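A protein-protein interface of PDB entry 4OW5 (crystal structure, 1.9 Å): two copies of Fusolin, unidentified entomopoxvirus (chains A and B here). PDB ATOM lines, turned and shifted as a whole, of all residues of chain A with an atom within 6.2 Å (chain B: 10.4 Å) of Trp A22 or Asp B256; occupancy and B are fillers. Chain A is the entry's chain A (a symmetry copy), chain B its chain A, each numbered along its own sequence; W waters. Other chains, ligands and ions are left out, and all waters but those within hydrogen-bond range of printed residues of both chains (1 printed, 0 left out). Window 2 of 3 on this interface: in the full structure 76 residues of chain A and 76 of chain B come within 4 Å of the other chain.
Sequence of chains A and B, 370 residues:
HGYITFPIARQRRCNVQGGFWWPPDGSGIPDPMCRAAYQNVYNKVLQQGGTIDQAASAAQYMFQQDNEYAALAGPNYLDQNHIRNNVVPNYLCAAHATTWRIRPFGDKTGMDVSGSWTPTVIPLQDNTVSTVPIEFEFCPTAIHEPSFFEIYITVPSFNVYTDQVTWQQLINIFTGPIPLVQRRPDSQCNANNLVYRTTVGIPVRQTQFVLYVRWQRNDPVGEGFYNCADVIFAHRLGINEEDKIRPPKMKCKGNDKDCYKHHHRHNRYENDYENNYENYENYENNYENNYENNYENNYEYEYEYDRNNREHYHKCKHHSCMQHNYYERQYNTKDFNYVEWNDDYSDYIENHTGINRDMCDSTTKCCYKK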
ATOM      1  N   GLY A  19      25.518   6.186  -3.401  1.00  0.00           N
ATOM      2  CA  GLY A  19      25.626   7.581  -3.015  1.00  0.00           C
ATOM      3  C   GLY A  19      25.896   8.502  -4.196  1.00  0.00           C
ATOM      4  O   GLY A  19      26.078   9.689  -3.980  1.00  0.00           O
ATOM      5  N   PHE A  20      25.902   7.987  -5.446  1.00  0.00           N
ATOM      6  CA  PHE A  20      26.262   8.764  -6.655  1.00  0.00           C
ATOM      7  C   PHE A  20      25.043   9.214  -7.482  1.00  0.00           C
ATOM      8  O   PHE A  20      25.181  10.084  -8.341  1.00  0.00           O
ATOM      9  CB  PHE A  20      27.199   7.937  -7.561  1.00  0.00           C
ATOM     10  CG  PHE A  20      26.569   6.717  -8.203  1.00  0.00           C
ATOM     11  CD1 PHE A  20      25.806   6.833  -9.353  1.00  0.00           C
ATOM     12  CD2 PHE A  20      26.735   5.456  -7.651  1.00  0.00           C
ATOM     13  CE1 PHE A  20      25.216   5.715  -9.938  1.00  0.00           C
ATOM     14  CE2 PHE A  20      26.156   4.343  -8.242  1.00  0.00           C
ATOM     15  CZ  PHE A  20      25.395   4.478  -9.383  1.00  0.00           C
ATOM     16  N   TRP A  21      23.874   8.600  -7.287  1.00  0.00           N
ATOM     17  CA  TRP A  21      22.691   9.032  -8.047  1.00  0.00           C
ATOM     18  C   TRP A  21      22.253  10.433  -7.650  1.00  0.00           C
ATOM     19  O   TRP A  21      21.661  11.142  -8.459  1.00  0.00           O
ATOM     20  CB  TRP A  21      21.510   8.060  -7.854  1.00  0.00           C
ATOM     21  CG  TRP A  21      21.681   6.747  -8.531  1.00  0.00           C
ATOM     22  CD1 TRP A  21      21.664   5.519  -7.948  1.00  0.00           C
ATOM     23  CD2 TRP A  21      21.876   6.528  -9.933  1.00  0.00           C
ATOM     24  NE1 TRP A  21      21.889   4.550  -8.898  1.00  0.00           N
ATOM     25  CE2 TRP A  21      21.940   5.135 -10.134  1.00  0.00           C
ATOM     26  CE3 TRP A  21      22.024   7.375 -11.035  1.00  0.00           C
ATOM     27  CZ2 TRP A  21      22.214   4.576 -11.390  1.00  0.00           C
ATOM     28  CZ3 TRP A  21      22.212   6.819 -12.287  1.00  0.00           C
ATOM     29  CH2 TRP A  21      22.303   5.434 -12.456  1.00  0.00           C
ATOM     30  N   TRP A  22      22.512  10.812  -6.404  1.00  0.00           N
ATOM     31  CA  TRP A  22      22.098  12.098  -5.865  1.00  0.00           C
ATOM     32  C   TRP A  22      22.878  12.395  -4.589  1.00  0.00           C
ATOM     33  O   TRP A  22      23.033  11.467  -3.793  1.00  0.00           O
ATOM     34  CB  TRP A  22      20.582  12.069  -5.546  1.00  0.00           C
ATOM     35  CG  TRP A  22      20.025  13.438  -5.353  1.00  0.00           C
ATOM     36  CD1 TRP A  22      19.982  14.143  -4.186  1.00  0.00           C
ATOM     37  CD2 TRP A  22      19.739  14.370  -6.396  1.00  0.00           C
ATOM     38  NE1 TRP A  22      19.603  15.438  -4.432  1.00  0.00           N
ATOM     39  CE2 TRP A  22      19.446  15.606  -5.784  1.00  0.00           C
ATOM     40  CE3 TRP A  22      19.703  14.280  -7.793  1.00  0.00           C
ATOM     41  CZ2 TRP A  22      19.125  16.745  -6.525  1.00  0.00           C
ATOM     42  CZ3 TRP A  22      19.325  15.393  -8.522  1.00  0.00           C
ATOM     43  CH2 TRP A  22      19.057  16.612  -7.891  1.00  0.00           C
ATOM     44  N   PRO A  23      23.340  13.624  -4.293  1.00  0.00           N
ATOM     45  CA  PRO A  23      23.334  14.853  -5.118  1.00  0.00           C
ATOM     46  C   PRO A  23      24.120  14.682  -6.432  1.00  0.00           C
ATOM     47  O   PRO A  23      24.968  13.789  -6.528  1.00  0.00           O
ATOM     48  CB  PRO A  23      24.006  15.895  -4.212  1.00  0.00           C
ATOM     49  CG  PRO A  23      24.069  15.306  -2.872  1.00  0.00           C
ATOM     50  CD  PRO A  23      24.074  13.834  -3.036  1.00  0.00           C
ATOM     51  N   PRO A  24      23.829  15.500  -7.463  1.00  0.00           N
ATOM     52  CA  PRO A  24      24.493  15.303  -8.767  1.00  0.00           C
ATOM     53  C   PRO A  24      25.995  15.567  -8.801  1.00  0.00           C
ATOM     54  O   PRO A  24      26.629  15.087  -9.714  1.00  0.00           O
ATOM     55  CB  PRO A  24      23.766  16.279  -9.707  1.00  0.00           C
ATOM     56  CG  PRO A  24      22.986  17.172  -8.862  1.00  0.00           C
ATOM     57  CD  PRO A  24      22.831  16.590  -7.514  1.00  0.00           C
ATOM     58  N   GLY A  26      28.212  14.356  -6.798  1.00  0.00           N
ATOM     59  CA  GLY A  26      28.932  13.237  -6.204  1.00  0.00           C
ATOM     60  C   GLY A  26      29.346  13.400  -4.768  1.00  0.00           C
ATOM     61  O   GLY A  26      30.033  12.523  -4.249  1.00  0.00           O
ATOM     62  N   GLY A  28      27.738  12.851  -2.159  1.00  0.00           N
ATOM     63  CA  GLY A  28      27.174  11.774  -1.351  1.00  0.00           C
ATOM     64  C   GLY A  28      27.971  10.483  -1.451  1.00  0.00           C
ATOM     65  O   GLY A  28      27.639   9.487  -0.798  1.00  0.00           O
ATOM     66  N   TYR A  38      34.274  10.151  -9.842  1.00  0.00           N
ATOM     67  CA  TYR A  38      33.007  10.755 -10.228  1.00  0.00           C
ATOM     68  C   TYR A  38      33.200  12.255 -10.543  1.00  0.00           C
ATOM     69  O   TYR A  38      32.829  12.735 -11.619  1.00  0.00           O
ATOM     70  CB  TYR A  38      31.973  10.570  -9.108  1.00  0.00           C
ATOM     71  CG  TYR A  38      30.599  11.107  -9.444  1.00  0.00           C
ATOM     72  CD1 TYR A  38      30.339  12.474  -9.430  1.00  0.00           C
ATOM     73  CD2 TYR A  38      29.557  10.247  -9.774  1.00  0.00           C
ATOM     74  CE1 TYR A  38      29.068  12.968  -9.724  1.00  0.00           C
ATOM     75  CE2 TYR A  38      28.295  10.727 -10.078  1.00  0.00           C
ATOM     76  CZ  TYR A  38      28.040  12.087 -10.003  1.00  0.00           C
ATOM     77  OH  TYR A  38      26.792  12.534 -10.306  1.00  0.00           O
ATOM     78  N   GLN A  60      27.547   9.722 -13.758  1.00  0.00           N
ATOM     79  CA  GLN A  60      26.686   8.619 -13.300  1.00  0.00           C
ATOM     80  C   GLN A  60      26.728   7.475 -14.302  1.00  0.00           C
ATOM     81  O   GLN A  60      26.706   6.322 -13.873  1.00  0.00           O
ATOM     82  CB  GLN A  60      25.240   9.060 -13.034  1.00  0.00           C
ATOM     83  CG  GLN A  60      25.163   9.962 -11.834  1.00  0.00           C
ATOM     84  CD  GLN A  60      23.835  10.623 -11.625  1.00  0.00           C
ATOM     85  OE1 GLN A  60      22.909  10.464 -12.404  1.00  0.00           O
ATOM     86  NE2 GLN A  60      23.738  11.393 -10.553  1.00  0.00           N
ATOM     87  N   CYS B 252      25.339  29.694  -9.201  1.00  0.00           N
ATOM     88  CA  CYS B 252      24.101  29.013  -9.574  1.00  0.00           C
ATOM     89  C   CYS B 252      22.965  29.454  -8.682  1.00  0.00           C
ATOM     90  O   CYS B 252      23.210  29.897  -7.561  1.00  0.00           O
ATOM     91  CB  CYS B 252      24.285  27.500  -9.490  1.00  0.00           C
ATOM     92  SG  CYS B 252      25.534  26.836 -10.617  1.00  0.00           S
ATOM     93  N   LYS B 253      21.719  29.257  -9.156  1.00  0.00           N
ATOM     94  CA  LYS B 253      20.518  29.574  -8.376  1.00  0.00           C
ATOM     95  C   LYS B 253      19.385  28.606  -8.724  1.00  0.00           C
ATOM     96  O   LYS B 253      19.380  28.012  -9.793  1.00  0.00           O
ATOM     97  CB  LYS B 253      20.078  31.037  -8.632  1.00  0.00           C
ATOM     98  CG  LYS B 253      19.514  31.253 -10.023  1.00  0.00           C
ATOM     99  CD  LYS B 253      19.279  32.717 -10.293  1.00  0.00           C
ATOM    100  CE  LYS B 253      18.519  32.907 -11.587  1.00  0.00           C
ATOM    101  NZ  LYS B 253      18.128  34.330 -11.778  1.00  0.00           N
ATOM    102  N   GLY B 254      18.410  28.503  -7.845  1.00  0.00           N
ATOM    103  CA  GLY B 254      17.267  27.624  -8.064  1.00  0.00           C
ATOM    104  C   GLY B 254      16.628  27.178  -6.775  1.00  0.00           C
ATOM    105  O   GLY B 254      17.213  27.339  -5.703  1.00  0.00           O
ATOM    106  N   ASN B 255      15.442  26.601  -6.882  1.00  0.00           N
ATOM    107  CA  ASN B 255      14.632  26.165  -5.724  1.00  0.00           C
ATOM    108  C   ASN B 255      15.158  24.902  -5.011  1.00  0.00           C
ATOM    109  O   ASN B 255      14.729  24.657  -3.884  1.00  0.00           O
ATOM    110  CB  ASN B 255      13.164  25.938  -6.130  1.00  0.00           C
ATOM    111  CG  ASN B 255      12.924  24.889  -7.206  1.00  0.00           C
ATOM    112  OD1 ASN B 255      13.768  24.026  -7.476  1.00  0.00           O
ATOM    113  ND2 ASN B 255      11.808  24.996  -7.919  1.00  0.00           N
ATOM    114  N   ASP B 256      16.022  24.082  -5.649  1.00  0.00           N
ATOM    115  CA  ASP B 256      16.576  22.888  -4.979  1.00  0.00           C
ATOM    116  C   ASP B 256      18.059  23.102  -4.707  1.00  0.00           C
ATOM    117  O   ASP B 256      18.874  22.999  -5.619  1.00  0.00           O
ATOM    118  CB  ASP B 256      16.337  21.615  -5.802  1.00  0.00           C
ATOM    119  CG  ASP B 256      16.768  20.320  -5.129  1.00  0.00           C
ATOM    120  OD1 ASP B 256      17.061  20.343  -3.901  1.00  0.00           O
ATOM    121  OD2 ASP B 256      16.765  19.283  -5.801  1.00  0.00           O
ATOM    122  N   LYS B 257      18.399  23.404  -3.438  1.00  0.00           N
ATOM    123  CA  LYS B 257      19.772  23.660  -2.992  1.00  0.00           C
ATOM    124  C   LYS B 257      20.745  22.488  -3.285  1.00  0.00           C
ATOM    125  O   LYS B 257      21.915  22.755  -3.494  1.00  0.00           O
ATOM    126  CB  LYS B 257      19.805  23.967  -1.480  1.00  0.00           C
ATOM    127  N   ASP B 258      20.275  21.216  -3.326  1.00  0.00           N
ATOM    128  CA  ASP B 258      21.159  20.065  -3.596  1.00  0.00           C
ATOM    129  C   ASP B 258      21.748  20.082  -5.022  1.00  0.00           C
ATOM    130  O   ASP B 258      22.740  19.395  -5.269  1.00  0.00           O
ATOM    131  CB  ASP B 258      20.419  18.734  -3.395  1.00  0.00           C
ATOM    132  CG  ASP B 258      19.985  18.422  -1.970  1.00  0.00           C
ATOM    133  OD1 ASP B 258      20.469  19.106  -1.031  1.00  0.00           O
ATOM    134  OD2 ASP B 258      19.168  17.487  -1.790  1.00  0.00           O
ATOM    135  N   CYS B 259      21.128  20.832  -5.951  1.00  0.00           N
ATOM    136  CA  CYS B 259      21.582  20.921  -7.338  1.00  0.00           C
ATOM    137  C   CYS B 259      22.936  21.639  -7.489  1.00  0.00           C
ATOM    138  O   CYS B 259      23.633  21.367  -8.458  1.00  0.00           O
ATOM    139  CB  CYS B 259      20.518  21.593  -8.207  1.00  0.00           C
ATOM    140  SG  CYS B 259      19.184  20.490  -8.723  1.00  0.00           S
ATOM    141  N   TYR B 260      23.311  22.544  -6.571  1.00  0.00           N
ATOM    142  CA  TYR B 260      24.549  23.321  -6.737  1.00  0.00           C
ATOM    143  C   TYR B 260      25.230  23.641  -5.409  1.00  0.00           C
ATOM    144  O   TYR B 260      24.578  23.644  -4.376  1.00  0.00           O
ATOM    145  CB  TYR B 260      24.228  24.631  -7.485  1.00  0.00           C
ATOM    146  CG  TYR B 260      23.089  25.423  -6.878  1.00  0.00           C
ATOM    147  CD1 TYR B 260      21.774  25.193  -7.258  1.00  0.00           C
ATOM    148  CD2 TYR B 260      23.328  26.402  -5.920  1.00  0.00           C
ATOM    149  CE1 TYR B 260      20.721  25.900  -6.686  1.00  0.00           C
ATOM    150  CE2 TYR B 260      22.281  27.115  -5.338  1.00  0.00           C
ATOM    151  CZ  TYR B 260      20.976  26.859  -5.721  1.00  0.00           C
ATOM    152  OH  TYR B 260      19.947  27.567  -5.143  1.00  0.00           O
ATOM    153  N   THR B 333      25.649   4.299   2.830  1.00  0.00           N
ATOM    154  CA  THR B 333      24.900   5.312   2.098  1.00  0.00           C
ATOM    155  C   THR B 333      23.440   4.971   2.263  1.00  0.00           C
ATOM    156  O   THR B 333      23.107   3.869   2.701  1.00  0.00           O
ATOM    157  CB  THR B 333      25.281   5.353   0.608  1.00  0.00           C
ATOM    158  OG1 THR B 333      24.957   4.108  -0.002  1.00  0.00           O
ATOM    159  CG2 THR B 333      26.698   5.666   0.405  1.00  0.00           C
ATOM    160  N   LYS B 334      22.579   5.854   1.796  1.00  0.00           N
ATOM    161  CA  LYS B 334      21.151   5.579   1.797  1.00  0.00           C
ATOM    162  C   LYS B 334      20.776   4.402   0.851  1.00  0.00           C
ATOM    163  O   LYS B 334      19.731   3.796   1.035  1.00  0.00           O
ATOM    164  CB  LYS B 334      20.367   6.826   1.401  1.00  0.00           C
ATOM    165  CG  LYS B 334      20.489   7.942   2.398  1.00  0.00           C
ATOM    166  CD  LYS B 334      19.633   9.137   1.974  1.00  0.00           C
ATOM    167  CE  LYS B 334      20.038  10.352   2.776  1.00  0.00           C
ATOM    168  NZ  LYS B 334      19.191  11.530   2.476  1.00  0.00           N
ATOM    169  N   ASP B 335      21.606   4.078  -0.153  1.00  0.00           N
ATOM    170  CA  ASP B 335      21.297   2.980  -1.064  1.00  0.00           C
ATOM    171  C   ASP B 335      22.290   1.816  -0.939  1.00  0.00           C
ATOM    172  O   ASP B 335      22.250   0.933  -1.770  1.00  0.00           O
ATOM    173  CB  ASP B 335      21.184   3.489  -2.509  1.00  0.00           C
ATOM    174  CG  ASP B 335      22.383   4.199  -3.046  1.00  0.00           C
ATOM    175  OD1 ASP B 335      23.256   4.581  -2.240  1.00  0.00           O
ATOM    176  OD2 ASP B 335      22.429   4.428  -4.267  1.00  0.00           O
HETATM  177  O   HOH W   1      16.549  17.095  -4.029  1.00  0.00           O
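The side-chain carboxylate (OD1) of Asp B335 is in hydrogen-bond range of the backbone NH (N) of Gly A19, at 3.0 Å.
The side-chain carboxylate (OD2) of Asp B258 lies within hydrogen-bond range of the indole nitrogen (NE1) of Trp A22, at 3.4 Å.
N of Asp B258 sits close to OD1 of Asp B256, 3.4 Å away.
OG1 of Thr B333 sits at hydrogen-bond distance from OD1 of Asp B335 (2.9 Å).
O of Pro A24 lies within hydrogen-bond range of OH of Tyr A38, 2.6 Å away.
The backbone carbonyl oxygen (O) of Trp A21 lies within hydrogen-bond range of the side-chain amide nitrogen (NE2) of Gln A60, at 3.0 Å.
Among the printed residues, pairs that only touch across the chains: Trp A21 with Asp B335 (3.9 Å), Trp A22 with Asp B256 (3.5 Å), Trp A22 with Cys B259 (3.97 Å), Pro A23 with Asp B258 (3.9 Å) and Pro A24 with Asp B258 (3.6 Å).
Of the printed residues of chain B, Gly A19 touches Asp B335 (3.0 Å).
Of chain B, only Asp B256 (3.5 Å), Asp B258 (3.4 Å) and Cys B259 (3.97 Å) come within 4 Å of Trp A22.
Of the printed residues of chain B, Pro A24 touches Asp B258 (3.6 Å).
No residue of chain B comes within 4 Å of Gly A28.
Of chain A, only Trp A22 (3.5 Å) comes within 4 Å of Asp B256.
Of the printed residues of chain A, Asp B258 touches Trp A22, Pro A23 and Pro A24.
Printed residues of chain A within 4 Å of Cys B259: Trp A22 (3.97 Å).
Of the printed residues of chain A, Asp B335 touches Gly A19 and Trp A21.
The nearest printed residue of chain B that does not touch Trp A21 is Thr B333 (8.6 Å).
Of the 10 printed residues of chain A, 5 touch a printed residue of chain B.
Printed residues of chain A that touch a printed residue of chain B: Gly A19, Trp A21, Trp A22, Pro A23 and Pro A24.
Hydrophobic or aromatic side chains of chain A within 4 Å of the printed part of chain B: Trp A21, Trp A22, Pro A23 and Pro A24.
Along chain A the printed residues that touch a printed residue of chain B span positions 19 to 24.
Of the 12 printed residues of chain B, 4 touch a printed residue of chain A.
Printed residues of chain B that touch a printed residue of chain A: Asp B256, Asp B258, Cys B259 and Asp B335.
Among the printed residues, 7 pairs touch across the chains.
Among the printed residues, no Asp or Glu carboxylate lies within 4 Å of a Lys or Arg side-chain nitrogen of the other chain.
No position is printed for both chains.
Of the 7 pairs that touch across the chains among the printed residues, none has its exchanged pair printed and touching as well.
Water W1 lies within hydrogen-bond range of the side-chain carboxylate (OD2) of Asp B256 (2.8 Å), the side-chain carboxylate (OD2) of Asp B258 (3.5 Å) and the indole nitrogen (NE1) of Trp A22 (3.5 Å).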
